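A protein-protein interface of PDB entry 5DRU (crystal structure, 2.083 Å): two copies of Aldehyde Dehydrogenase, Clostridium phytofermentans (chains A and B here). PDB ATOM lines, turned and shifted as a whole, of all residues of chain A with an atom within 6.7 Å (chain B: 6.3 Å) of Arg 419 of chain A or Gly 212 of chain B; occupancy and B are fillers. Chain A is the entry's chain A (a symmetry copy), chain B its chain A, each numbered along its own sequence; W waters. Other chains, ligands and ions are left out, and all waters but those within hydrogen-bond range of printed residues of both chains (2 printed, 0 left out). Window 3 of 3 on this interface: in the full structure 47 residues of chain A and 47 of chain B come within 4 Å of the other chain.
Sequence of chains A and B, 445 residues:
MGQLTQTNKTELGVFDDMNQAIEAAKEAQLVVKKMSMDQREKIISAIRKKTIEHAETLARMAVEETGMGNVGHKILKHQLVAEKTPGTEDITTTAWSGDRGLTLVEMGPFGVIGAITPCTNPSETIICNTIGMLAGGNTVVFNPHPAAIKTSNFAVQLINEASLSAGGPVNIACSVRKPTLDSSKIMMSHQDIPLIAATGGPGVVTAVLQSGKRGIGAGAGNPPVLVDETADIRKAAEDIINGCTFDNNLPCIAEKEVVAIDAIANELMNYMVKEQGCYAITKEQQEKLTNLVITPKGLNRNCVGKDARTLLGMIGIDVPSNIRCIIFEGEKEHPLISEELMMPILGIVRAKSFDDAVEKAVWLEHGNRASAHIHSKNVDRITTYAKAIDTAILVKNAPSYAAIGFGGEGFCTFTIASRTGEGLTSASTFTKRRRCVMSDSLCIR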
ATOM      1  N   GLY A 201       4.032 -34.087   7.190  1.00  0.00           N
ATOM      2  CA  GLY A 201       4.444 -32.942   7.996  1.00  0.00           C
ATOM      3  C   GLY A 201       4.942 -31.749   7.191  1.00  0.00           C
ATOM      4  O   GLY A 201       4.993 -31.765   5.959  1.00  0.00           O
ATOM      5  N   PRO A 202       5.316 -30.681   7.892  1.00  0.00           N
ATOM      6  CA  PRO A 202       5.669 -29.440   7.193  1.00  0.00           C
ATOM      7  C   PRO A 202       6.953 -29.583   6.388  1.00  0.00           C
ATOM      8  O   PRO A 202       7.132 -28.880   5.392  1.00  0.00           O
ATOM      9  CB  PRO A 202       5.829 -28.423   8.332  1.00  0.00           C
ATOM     10  CG  PRO A 202       6.081 -29.219   9.539  1.00  0.00           C
ATOM     11  CD  PRO A 202       5.346 -30.532   9.349  1.00  0.00           C
ATOM     12  N   GLY A 203       7.813 -30.512   6.795  1.00  0.00           N
ATOM     13  CA  GLY A 203       9.092 -30.694   6.138  1.00  0.00           C
ATOM     14  C   GLY A 203       8.931 -31.087   4.684  1.00  0.00           C
ATOM     15  O   GLY A 203       9.582 -30.542   3.792  1.00  0.00           O
ATOM     16  N   VAL A 204       8.058 -32.057   4.453  1.00  0.00           N
ATOM     17  CA  VAL A 204       7.851 -32.613   3.123  1.00  0.00           C
ATOM     18  C   VAL A 204       7.004 -31.670   2.266  1.00  0.00           C
ATOM     19  O   VAL A 204       7.177 -31.577   1.049  1.00  0.00           O
ATOM     20  CB  VAL A 204       7.173 -34.010   3.204  1.00  0.00           C
ATOM     21  CG1 VAL A 204       5.844 -33.936   3.956  1.00  0.00           C
ATOM     22  CG2 VAL A 204       7.006 -34.600   1.814  1.00  0.00           C
ATOM     23  N   VAL A 205       6.082 -30.969   2.906  1.00  0.00           N
ATOM     24  CA  VAL A 205       5.228 -30.075   2.181  1.00  0.00           C
ATOM     25  C   VAL A 205       6.060 -28.925   1.684  1.00  0.00           C
ATOM     26  O   VAL A 205       5.987 -28.560   0.511  1.00  0.00           O
ATOM     27  CB  VAL A 205       4.103 -29.575   3.040  1.00  0.00           C
ATOM     28  CG1 VAL A 205       3.277 -28.528   2.279  1.00  0.00           C
ATOM     29  CG2 VAL A 205       3.254 -30.759   3.493  1.00  0.00           C
ATOM     30  N   THR A 206       6.860 -28.353   2.581  1.00  0.00           N
ATOM     31  CA  THR A 206       7.725 -27.248   2.204  1.00  0.00           C
ATOM     32  C   THR A 206       8.589 -27.660   1.027  1.00  0.00           C
ATOM     33  O   THR A 206       8.855 -26.856   0.141  1.00  0.00           O
ATOM     34  CB  THR A 206       8.637 -26.795   3.344  1.00  0.00           C
ATOM     35  OG1 THR A 206       7.832 -26.282   4.396  1.00  0.00           O
ATOM     36  CG2 THR A 206       9.582 -25.689   2.874  1.00  0.00           C
ATOM     37  N   ALA A 207       9.012 -28.921   1.025  1.00  0.00           N
ATOM     38  CA  ALA A 207       9.963 -29.379   0.036  1.00  0.00           C
ATOM     39  C   ALA A 207       9.282 -29.491  -1.310  1.00  0.00           C
ATOM     40  O   ALA A 207       9.921 -29.244  -2.328  1.00  0.00           O
ATOM     41  CB  ALA A 207      10.583 -30.707   0.442  1.00  0.00           C
ATOM     42  N   VAL A 208       7.995 -29.837  -1.331  1.00  0.00           N
ATOM     43  CA  VAL A 208       7.337 -29.966  -2.625  1.00  0.00           C
ATOM     44  C   VAL A 208       7.019 -28.581  -3.195  1.00  0.00           C
ATOM     45  O   VAL A 208       6.907 -28.431  -4.396  1.00  0.00           O
ATOM     46  CB  VAL A 208       6.047 -30.825  -2.572  1.00  0.00           C
ATOM     47  CG1 VAL A 208       6.325 -32.170  -1.890  1.00  0.00           C
ATOM     48  CG2 VAL A 208       4.870 -30.096  -1.920  1.00  0.00           C
ATOM     49  N   LEU A 209       6.878 -27.579  -2.337  1.00  0.00           N
ATOM     50  CA  LEU A 209       6.531 -26.255  -2.806  1.00  0.00           C
ATOM     51  C   LEU A 209       7.780 -25.513  -3.217  1.00  0.00           C
ATOM     52  O   LEU A 209       7.714 -24.339  -3.565  1.00  0.00           O
ATOM     53  CB  LEU A 209       5.776 -25.478  -1.742  1.00  0.00           C
ATOM     54  CG  LEU A 209       4.391 -26.059  -1.489  1.00  0.00           C
ATOM     55  CD1 LEU A 209       3.994 -25.570  -0.130  1.00  0.00           C
ATOM     56  CD2 LEU A 209       3.393 -25.671  -2.574  1.00  0.00           C
ATOM     57  N   GLN A 210       8.916 -26.218  -3.145  1.00  0.00           N
ATOM     58  CA  GLN A 210      10.194 -25.748  -3.658  1.00  0.00           C
ATOM     59  C   GLN A 210      10.614 -26.534  -4.878  1.00  0.00           C
ATOM     60  O   GLN A 210      11.745 -26.388  -5.363  1.00  0.00           O
ATOM     61  CB  GLN A 210      11.301 -25.858  -2.601  1.00  0.00           C
ATOM     62  CG  GLN A 210      11.023 -25.039  -1.381  1.00  0.00           C
ATOM     63  CD  GLN A 210      12.069 -25.223  -0.285  1.00  0.00           C
ATOM     64  OE1 GLN A 210      12.818 -26.213  -0.270  1.00  0.00           O
ATOM     65  NE2 GLN A 210      12.125 -24.263   0.641  1.00  0.00           N
ATOM     66  N   SER A 211       9.729 -27.386  -5.371  1.00  0.00           N
ATOM     67  CA  SER A 211      10.108 -28.300  -6.449  1.00  0.00           C
ATOM     68  C   SER A 211      10.066 -27.697  -7.872  1.00  0.00           C
ATOM     69  O   SER A 211      10.690 -28.234  -8.799  1.00  0.00           O
ATOM     70  CB  SER A 211       9.200 -29.520  -6.381  1.00  0.00           C
ATOM     71  OG  SER A 211       7.875 -29.133  -6.626  1.00  0.00           O
ATOM     72  N   GLY A 217      -0.554 -29.071  -0.714  1.00  0.00           N
ATOM     73  CA  GLY A 217       0.198 -29.214   0.509  1.00  0.00           C
ATOM     74  C   GLY A 217      -0.701 -29.468   1.697  1.00  0.00           C
ATOM     75  O   GLY A 217      -1.452 -28.598   2.130  1.00  0.00           O
ATOM     76  N   ALA A 218      -0.629 -30.673   2.241  1.00  0.00           N
ATOM     77  CA  ALA A 218      -1.422 -30.999   3.417  1.00  0.00           C
ATOM     78  C   ALA A 218      -0.566 -30.937   4.663  1.00  0.00           C
ATOM     79  O   ALA A 218      -0.027 -31.970   5.072  1.00  0.00           O
ATOM     80  CB  ALA A 218      -2.061 -32.384   3.258  1.00  0.00           C
ATOM     81  N   GLY A 219      -0.468 -29.742   5.261  1.00  0.00           N
ATOM     82  CA  GLY A 219       0.361 -29.490   6.439  1.00  0.00           C
ATOM     83  C   GLY A 219      -0.203 -30.016   7.751  1.00  0.00           C
ATOM     84  O   GLY A 219      -1.227 -30.681   7.766  1.00  0.00           O
ATOM     85  N   ALA A 220       0.461 -29.720   8.863  1.00  0.00           N
ATOM     86  CA  ALA A 220       0.051 -30.279  10.152  1.00  0.00           C
ATOM     87  C   ALA A 220      -0.907 -29.365  10.907  1.00  0.00           C
ATOM     88  O   ALA A 220      -1.316 -28.315  10.403  1.00  0.00           O
ATOM     89  CB  ALA A 220       1.266 -30.579  11.013  1.00  0.00           C
ATOM     90  N   ASN A 368      -2.132 -22.787  11.980  1.00  0.00           N
ATOM     91  CA  ASN A 368      -2.122 -23.799  10.927  1.00  0.00           C
ATOM     92  C   ASN A 368      -3.337 -23.681   9.988  1.00  0.00           C
ATOM     93  O   ASN A 368      -3.282 -24.122   8.838  1.00  0.00           O
ATOM     94  CB  ASN A 368      -2.070 -25.200  11.542  1.00  0.00           C
ATOM     95  CG  ASN A 368      -0.650 -25.603  12.027  1.00  0.00           C
ATOM     96  OD1 ASN A 368      -0.464 -26.089  13.140  1.00  0.00           O
ATOM     97  ND2 ASN A 368       0.332 -25.419  11.174  1.00  0.00           N
ATOM     98  N   ARG A 369      -4.447 -23.167  10.516  1.00  0.00           N
ATOM     99  CA  ARG A 369      -5.715 -23.090   9.787  1.00  0.00           C
ATOM    100  C   ARG A 369      -6.040 -24.491   9.194  1.00  0.00           C
ATOM    101  O   ARG A 369      -6.436 -24.635   8.015  1.00  0.00           O
ATOM    102  CB  ARG A 369      -5.646 -21.952   8.718  1.00  0.00           C
ATOM    103  CG  ARG A 369      -5.311 -20.563   9.355  1.00  0.00           C
ATOM    104  CD  ARG A 369      -5.828 -19.333   8.495  1.00  0.00           C
ATOM    105  NE  ARG A 369      -5.028 -19.087   7.294  1.00  0.00           N
ATOM    106  CZ  ARG A 369      -5.364 -18.263   6.301  1.00  0.00           C
ATOM    107  NH1 ARG A 369      -4.541 -18.101   5.266  1.00  0.00           N
ATOM    108  NH2 ARG A 369      -6.523 -17.612   6.324  1.00  0.00           N
ATOM    109  N   ILE A 416      -5.984 -33.397   3.235  1.00  0.00           N
ATOM    110  CA  ILE A 416      -6.621 -32.132   3.562  1.00  0.00           C
ATOM    111  C   ILE A 416      -5.604 -31.040   3.323  1.00  0.00           C
ATOM    112  O   ILE A 416      -4.657 -30.862   4.101  1.00  0.00           O
ATOM    113  CB  ILE A 416      -7.102 -32.103   5.015  1.00  0.00           C
ATOM    114  CG1 ILE A 416      -8.174 -33.184   5.212  1.00  0.00           C
ATOM    115  CG2 ILE A 416      -7.625 -30.729   5.384  1.00  0.00           C
ATOM    116  CD1 ILE A 416      -8.177 -33.816   6.597  1.00  0.00           C
ATOM    117  N   ALA A 417      -5.764 -30.318   2.230  1.00  0.00           N
ATOM    118  CA  ALA A 417      -4.675 -29.377   1.823  1.00  0.00           C
ATOM    119  C   ALA A 417      -4.760 -28.013   2.498  1.00  0.00           C
ATOM    120  O   ALA A 417      -5.041 -27.014   1.836  1.00  0.00           O
ATOM    121  CB  ALA A 417      -4.669 -29.201   0.309  1.00  0.00           C
ATOM    122  N   SER A 418      -4.430 -27.953   3.795  1.00  0.00           N
ATOM    123  CA  SER A 418      -4.687 -26.748   4.589  1.00  0.00           C
ATOM    124  C   SER A 418      -3.739 -25.611   4.262  1.00  0.00           C
ATOM    125  O   SER A 418      -4.116 -24.442   4.366  1.00  0.00           O
ATOM    126  CB  SER A 418      -4.614 -27.073   6.092  1.00  0.00           C
ATOM    127  OG  SER A 418      -3.369 -27.646   6.442  1.00  0.00           O
ATOM    128  N   ARG A 419      -2.519 -25.955   3.856  1.00  0.00           N
ATOM    129  CA  ARG A 419      -1.476 -24.995   3.597  1.00  0.00           C
ATOM    130  C   ARG A 419      -1.628 -24.229   2.272  1.00  0.00           C
ATOM    131  O   ARG A 419      -1.477 -23.019   2.244  1.00  0.00           O
ATOM    132  CB  ARG A 419      -0.134 -25.717   3.629  1.00  0.00           C
ATOM    133  CG  ARG A 419       1.072 -24.775   3.562  1.00  0.00           C
ATOM    134  CD  ARG A 419       2.253 -25.449   4.237  1.00  0.00           C
ATOM    135  NE  ARG A 419       3.531 -24.906   3.808  1.00  0.00           N
ATOM    136  CZ  ARG A 419       4.691 -25.534   3.926  1.00  0.00           C
ATOM    137  NH1 ARG A 419       4.750 -26.743   4.464  1.00  0.00           N
ATOM    138  NH2 ARG A 419       5.795 -24.944   3.494  1.00  0.00           N
ATOM    139  N   THR A 420      -1.924 -24.954   1.195  1.00  0.00           N
ATOM    140  CA  THR A 420      -1.957 -24.425  -0.155  1.00  0.00           C
ATOM    141  C   THR A 420      -3.374 -24.107  -0.567  1.00  0.00           C
ATOM    142  O   THR A 420      -3.598 -23.525  -1.628  1.00  0.00           O
ATOM    143  CB  THR A 420      -1.331 -25.424  -1.151  1.00  0.00           C
ATOM    144  OG1 THR A 420      -2.022 -26.670  -1.089  1.00  0.00           O
ATOM    145  CG2 THR A 420       0.116 -25.647  -0.824  1.00  0.00           C
ATOM    146  N   GLY A 421      -4.334 -24.532   0.264  1.00  0.00           N
ATOM    147  CA  GLY A 421      -5.673 -23.967   0.269  1.00  0.00           C
ATOM    148  C   GLY A 421      -6.812 -24.671  -0.437  1.00  0.00           C
ATOM    149  O   GLY A 421      -7.941 -24.165  -0.453  1.00  0.00           O
ATOM    150  N   GLU A 422      -6.549 -25.861  -0.964  1.00  0.00           N
ATOM    151  CA  GLU A 422      -7.555 -26.593  -1.715  1.00  0.00           C
ATOM    152  C   GLU A 422      -8.534 -27.310  -0.757  1.00  0.00           C
ATOM    153  O   GLU A 422      -9.600 -27.751  -1.157  1.00  0.00           O
ATOM    154  CB  GLU A 422      -6.868 -27.583  -2.669  1.00  0.00           C
ATOM    155  CG  GLU A 422      -5.976 -26.911  -3.772  1.00  0.00           C
ATOM    156  CD  GLU A 422      -4.485 -26.640  -3.353  1.00  0.00           C
ATOM    157  OE1 GLU A 422      -4.106 -26.896  -2.181  1.00  0.00           O
ATOM    158  OE2 GLU A 422      -3.655 -26.195  -4.210  1.00  0.00           O
ATOM    159  N   PHE B 110      -7.016 -15.901   1.665  1.00  0.00           N
ATOM    160  CA  PHE B 110      -5.621 -16.277   1.962  1.00  0.00           C
ATOM    161  C   PHE B 110      -4.920 -15.343   2.942  1.00  0.00           C
ATOM    162  O   PHE B 110      -4.352 -15.802   3.962  1.00  0.00           O
ATOM    163  CB  PHE B 110      -4.803 -16.307   0.684  1.00  0.00           C
ATOM    164  CG  PHE B 110      -4.636 -17.640   0.131  1.00  0.00           C
ATOM    165  CD1 PHE B 110      -3.647 -18.511   0.614  1.00  0.00           C
ATOM    166  CD2 PHE B 110      -5.446 -18.039  -0.889  1.00  0.00           C
ATOM    167  CE1 PHE B 110      -3.488 -19.775   0.064  1.00  0.00           C
ATOM    168  CE2 PHE B 110      -5.319 -19.343  -1.431  1.00  0.00           C
ATOM    169  CZ  PHE B 110      -4.332 -20.179  -0.969  1.00  0.00           C
ATOM    170  N   MET B 188       9.051 -13.393  -2.098  1.00  0.00           N
ATOM    171  CA  MET B 188       8.944 -14.839  -2.252  1.00  0.00           C
ATOM    172  C   MET B 188       9.479 -15.603  -1.061  1.00  0.00           C
ATOM    173  O   MET B 188       9.370 -16.830  -1.004  1.00  0.00           O
ATOM    174  CB  MET B 188       9.699 -15.307  -3.488  1.00  0.00           C
ATOM    175  CG  MET B 188       9.059 -14.928  -4.816  1.00  0.00           C
ATOM    176  SD  MET B 188       9.965 -15.636  -6.204  1.00  0.00           S
ATOM    177  CE  MET B 188      11.508 -16.198  -5.460  1.00  0.00           C
ATOM    178  N   PRO B 194       1.332 -16.062   1.838  1.00  0.00           N
ATOM    179  CA  PRO B 194       1.213 -17.506   1.575  1.00  0.00           C
ATOM    180  C   PRO B 194       0.983 -17.827   0.106  1.00  0.00           C
ATOM    181  O   PRO B 194       1.240 -18.940  -0.233  1.00  0.00           O
ATOM    182  CB  PRO B 194      -0.002 -17.924   2.417  1.00  0.00           C
ATOM    183  CG  PRO B 194      -0.864 -16.650   2.405  1.00  0.00           C
ATOM    184  CD  PRO B 194       0.129 -15.521   2.483  1.00  0.00           C
ATOM    185  N   VAL B 208       8.595 -18.766  -8.672  1.00  0.00           N
ATOM    186  CA  VAL B 208       7.622 -18.689  -7.590  1.00  0.00           C
ATOM    187  C   VAL B 208       7.257 -20.096  -7.108  1.00  0.00           C
ATOM    188  O   VAL B 208       6.853 -20.262  -5.974  1.00  0.00           O
ATOM    189  CB  VAL B 208       6.338 -17.911  -7.976  1.00  0.00           C
ATOM    190  CG1 VAL B 208       6.695 -16.546  -8.576  1.00  0.00           C
ATOM    191  CG2 VAL B 208       5.413 -18.707  -8.900  1.00  0.00           C
ATOM    192  N   LEU B 209       7.401 -21.097  -7.966  1.00  0.00           N
ATOM    193  CA  LEU B 209       7.029 -22.444  -7.590  1.00  0.00           C
ATOM    194  C   LEU B 209       8.177 -23.110  -6.868  1.00  0.00           C
ATOM    195  O   LEU B 209       8.097 -24.289  -6.540  1.00  0.00           O
ATOM    196  CB  LEU B 209       6.620 -23.258  -8.804  1.00  0.00           C
ATOM    197  CG  LEU B 209       5.312 -22.763  -9.406  1.00  0.00           C
ATOM    198  CD1 LEU B 209       5.304 -23.264 -10.818  1.00  0.00           C
ATOM    199  CD2 LEU B 209       4.097 -23.221  -8.608  1.00  0.00           C
ATOM    200  N   GLN B 210       9.247 -22.336  -6.655  1.00  0.00           N
ATOM    201  CA  GLN B 210      10.380 -22.729  -5.830  1.00  0.00           C
ATOM    202  C   GLN B 210      10.426 -21.928  -4.549  1.00  0.00           C
ATOM    203  O   GLN B 210      11.402 -22.007  -3.791  1.00  0.00           O
ATOM    204  CB  GLN B 210      11.710 -22.541  -6.571  1.00  0.00           C
ATOM    205  CG  GLN B 210      11.803 -23.366  -7.815  1.00  0.00           C
ATOM    206  CD  GLN B 210      13.080 -23.109  -8.610  1.00  0.00           C
ATOM    207  OE1 GLN B 210      13.745 -22.074  -8.442  1.00  0.00           O
ATOM    208  NE2 GLN B 210      13.430 -24.056  -9.483  1.00  0.00           N
ATOM    209  N   SER B 211       9.393 -21.137  -4.305  1.00  0.00           N
ATOM    210  CA  SER B 211       9.428 -20.210  -3.173  1.00  0.00           C
ATOM    211  C   SER B 211       9.063 -20.826  -1.802  1.00  0.00           C
ATOM    212  O   SER B 211       9.395 -20.259  -0.752  1.00  0.00           O
ATOM    213  CB  SER B 211       8.492 -19.048  -3.480  1.00  0.00           C
ATOM    214  OG  SER B 211       7.176 -19.519  -3.577  1.00  0.00           O
ATOM    215  N   GLY B 212       8.386 -21.973  -1.797  1.00  0.00           N
ATOM    216  CA  GLY B 212       7.952 -22.571  -0.540  1.00  0.00           C
ATOM    217  C   GLY B 212       6.524 -22.170  -0.194  1.00  0.00           C
ATOM    218  O   GLY B 212       5.958 -22.579   0.825  1.00  0.00           O
ATOM    219  N   LYS B 213       5.965 -21.338  -1.056  1.00  0.00           N
ATOM    220  CA  LYS B 213       4.576 -20.941  -1.023  1.00  0.00           C
ATOM    221  C   LYS B 213       3.846 -21.552  -2.224  1.00  0.00           C
ATOM    222  O   LYS B 213       4.468 -21.965  -3.230  1.00  0.00           O
ATOM    223  CB  LYS B 213       4.451 -19.413  -1.082  1.00  0.00           C
ATOM    224  CG  LYS B 213       5.083 -18.706   0.062  1.00  0.00           C
ATOM    225  CD  LYS B 213       5.653 -17.384  -0.389  1.00  0.00           C
ATOM    226  CE  LYS B 213       6.379 -16.726   0.744  1.00  0.00           C
ATOM    227  NZ  LYS B 213       6.838 -17.724   1.735  1.00  0.00           N
ATOM    228  N   ARG B 214       2.525 -21.593  -2.126  1.00  0.00           N
ATOM    229  CA  ARG B 214       1.730 -21.902  -3.288  1.00  0.00           C
ATOM    230  C   ARG B 214       1.929 -20.824  -4.333  1.00  0.00           C
ATOM    231  O   ARG B 214       1.792 -19.646  -4.030  1.00  0.00           O
ATOM    232  CB  ARG B 214       0.258 -21.977  -2.963  1.00  0.00           C
ATOM    233  CG  ARG B 214      -0.496 -22.420  -4.172  1.00  0.00           C
ATOM    234  CD  ARG B 214      -1.881 -22.713  -3.899  1.00  0.00           C
ATOM    235  NE  ARG B 214      -2.595 -22.807  -5.178  1.00  0.00           N
ATOM    236  CZ  ARG B 214      -3.913 -22.911  -5.241  1.00  0.00           C
ATOM    237  NH1 ARG B 214      -4.566 -22.871  -4.125  1.00  0.00           N
ATOM    238  NH2 ARG B 214      -4.569 -22.942  -6.408  1.00  0.00           N
ATOM    239  N   LYS B 432      -9.018 -19.803   0.087  1.00  0.00           N
ATOM    240  CA  LYS B 432      -8.903 -21.107   0.736  1.00  0.00           C
ATOM    241  C   LYS B 432     -10.285 -21.720   1.016  1.00  0.00           C
ATOM    242  O   LYS B 432     -11.210 -21.038   1.457  1.00  0.00           O
ATOM    243  CB  LYS B 432      -8.137 -20.991   2.050  1.00  0.00           C
ATOM    244  CG  LYS B 432      -6.816 -20.253   1.921  1.00  0.00           C
ATOM    245  CD  LYS B 432      -5.853 -20.428   3.104  1.00  0.00           C
ATOM    246  CE  LYS B 432      -5.480 -21.892   3.311  1.00  0.00           C
ATOM    247  NZ  LYS B 432      -4.630 -22.011   4.521  1.00  0.00           N
HETATM  248  O   HOH W   1      -1.057 -25.790  -4.845  1.00  0.00           O
HETATM  249  O   HOH W   2      -7.078 -23.420   5.504  1.00  0.00           O
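OG of Ser 211 of chain B is in hydrogen-bond range of O of Val 208 of chain B (2.5 Å). The side-chain hydroxyl of Ser 211 of chain B lies close to the backbone NH of Lys 213 of chain B, at 3.3 Å. O of Pro 202 of chain A is in hydrogen-bond range of NH1 of Arg 419 of chain A, at 3.3 Å. The guanidinium group (NH2) of Arg 419 of chain A lies within hydrogen-bond range of the side-chain hydroxyl (OG1) of Thr 206 of chain A, 2.6 Å away. OG of Ser 211 of chain A lies within hydrogen-bond range of O of Val 208 of chain A (2.5 Å). N of Ser 418 of chain A is in hydrogen-bond range of O of Gly 217 of chain A (3.5 Å).
Leu 209 of chain A touches its own counterpart, Leu 209 of chain B. Leu 209 of chain A touches Gln 210 of chain B, and with the chains exchanged Gln 210 of chain A touches Leu 209 of chain B. Leu 209 of chain A touches Ser 211 of chain B, and with the chains exchanged Ser 211 of chain A touches Leu 209 of chain B. Gln 210 of chain B touches its own counterpart, Gln 210 of chain A. Positions printed for both chains: 208, 209, 210 and 211.
Water W1 lies within hydrogen-bond range of the side-chain carboxylate (OE2) of Glu 422 of chain A and the guanidinium group (NE) of Arg 214 of chain B. Water W2 lies within hydrogen-bond range of the backbone carbonyl oxygen (O) of Arg 369 of chain A, the side-chain amino group (NZ) of Lys 432 of chain B and the backbone carbonyl oxygen (O) of Ser 418 of chain A.
Gln 210 of chain B touches Leu 209 of chain A. O of Leu 209 of chain A touches N of Ser 211 of chain B, at 3.7 Å. CD2 of Leu 209 of chain A touches O of Lys 213 of chain B, at 3.9 Å. C of Gln 210 of chain A touches O of Leu 209 of chain B (3.8 Å). Gln 210 of chain A touches Gln 210 of chain B. N of Ser 211 of chain A touches O of Leu 209 of chain B, at 3.7 Å. Lys 432 of chain B touches Arg 369 of chain A (CD to NH1, 3.4 Å). O of Gly 212 of chain B touches NH2 of Arg 419 of chain A, at 3.6 Å. Phe 110 of chain B touches Thr 420 of chain A. Gly 421 of chain A touches Lys 432 of chain B (O to CA, 3.4 Å).
O of Phe 110 of chain B lies within hydrogen-bond range of NH1 of Arg 369 of chain A. The backbone NH of Gly 212 of chain B is in hydrogen-bond range of the backbone carbonyl oxygen of Leu 209 of chain A (3.0 Å). The guanidinium group (NH1) of Arg 214 of chain B lies within hydrogen-bond range of the backbone carbonyl oxygen (O) of Thr 420 of chain A. The guanidinium group (NH1) of Arg 214 of chain B is in salt-bridge range of the side-chain carboxylate (OE2) of Glu 422 of chain A (3.4 Å). NZ of Lys 432 of chain B lies within hydrogen-bond range of O of Ser 418 of chain A (2.5 Å). O of Leu 209 of chain B sits close to O of Leu 209 of chain A (3.0 Å).
Of the printed residues of chain B, Arg 419 of chain A touches Gly 212 (3.6 Å). Gly 212 of chain B touches just these residues of chain A: Leu 209 (3.0 Å) and Arg 419 (3.6 Å). Of the printed residues of chain B, Ser 211 of chain A touches Leu 209. Printed residues of chain A within 4 Å of Lys 432 of chain B: Arg 369, Ser 418 and Gly 421. Of the printed residues of chain B, Glu 422 of chain A touches Arg 214 (3.4 Å). Of the printed residues of chain A, Arg 214 of chain B touches Thr 420 (2.8 Å) and Glu 422 (3.4 Å). Printed residues of chain B within 4 Å of Gly 421 of chain A: Lys 432 (3.4 Å). Val 204 of chain A touches none of the printed residues of chain B. The nearest printed residue of chain B that does not touch Arg 419 of chain A is Lys 432 of chain B (4.02 Å). The nearest residue of chain A that does not touch Gly 212 of chain B is Gln 210 of chain A (4.03 Å). The nearest printed residue of chain A that does not touch Ser 211 of chain B is Gln 210 of chain A (4.7 Å).
Of the 24 printed residues of chain A, 9 touch a printed residue of chain B. Hydrophobic or aromatic side chains of chain A within 4 Å of the printed part of chain B: Leu 209. Hydrophobic or aromatic side chains of chain B that line the printed part of chain A: Phe 110. Among the printed residues, 16 pairs touch across the chains.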
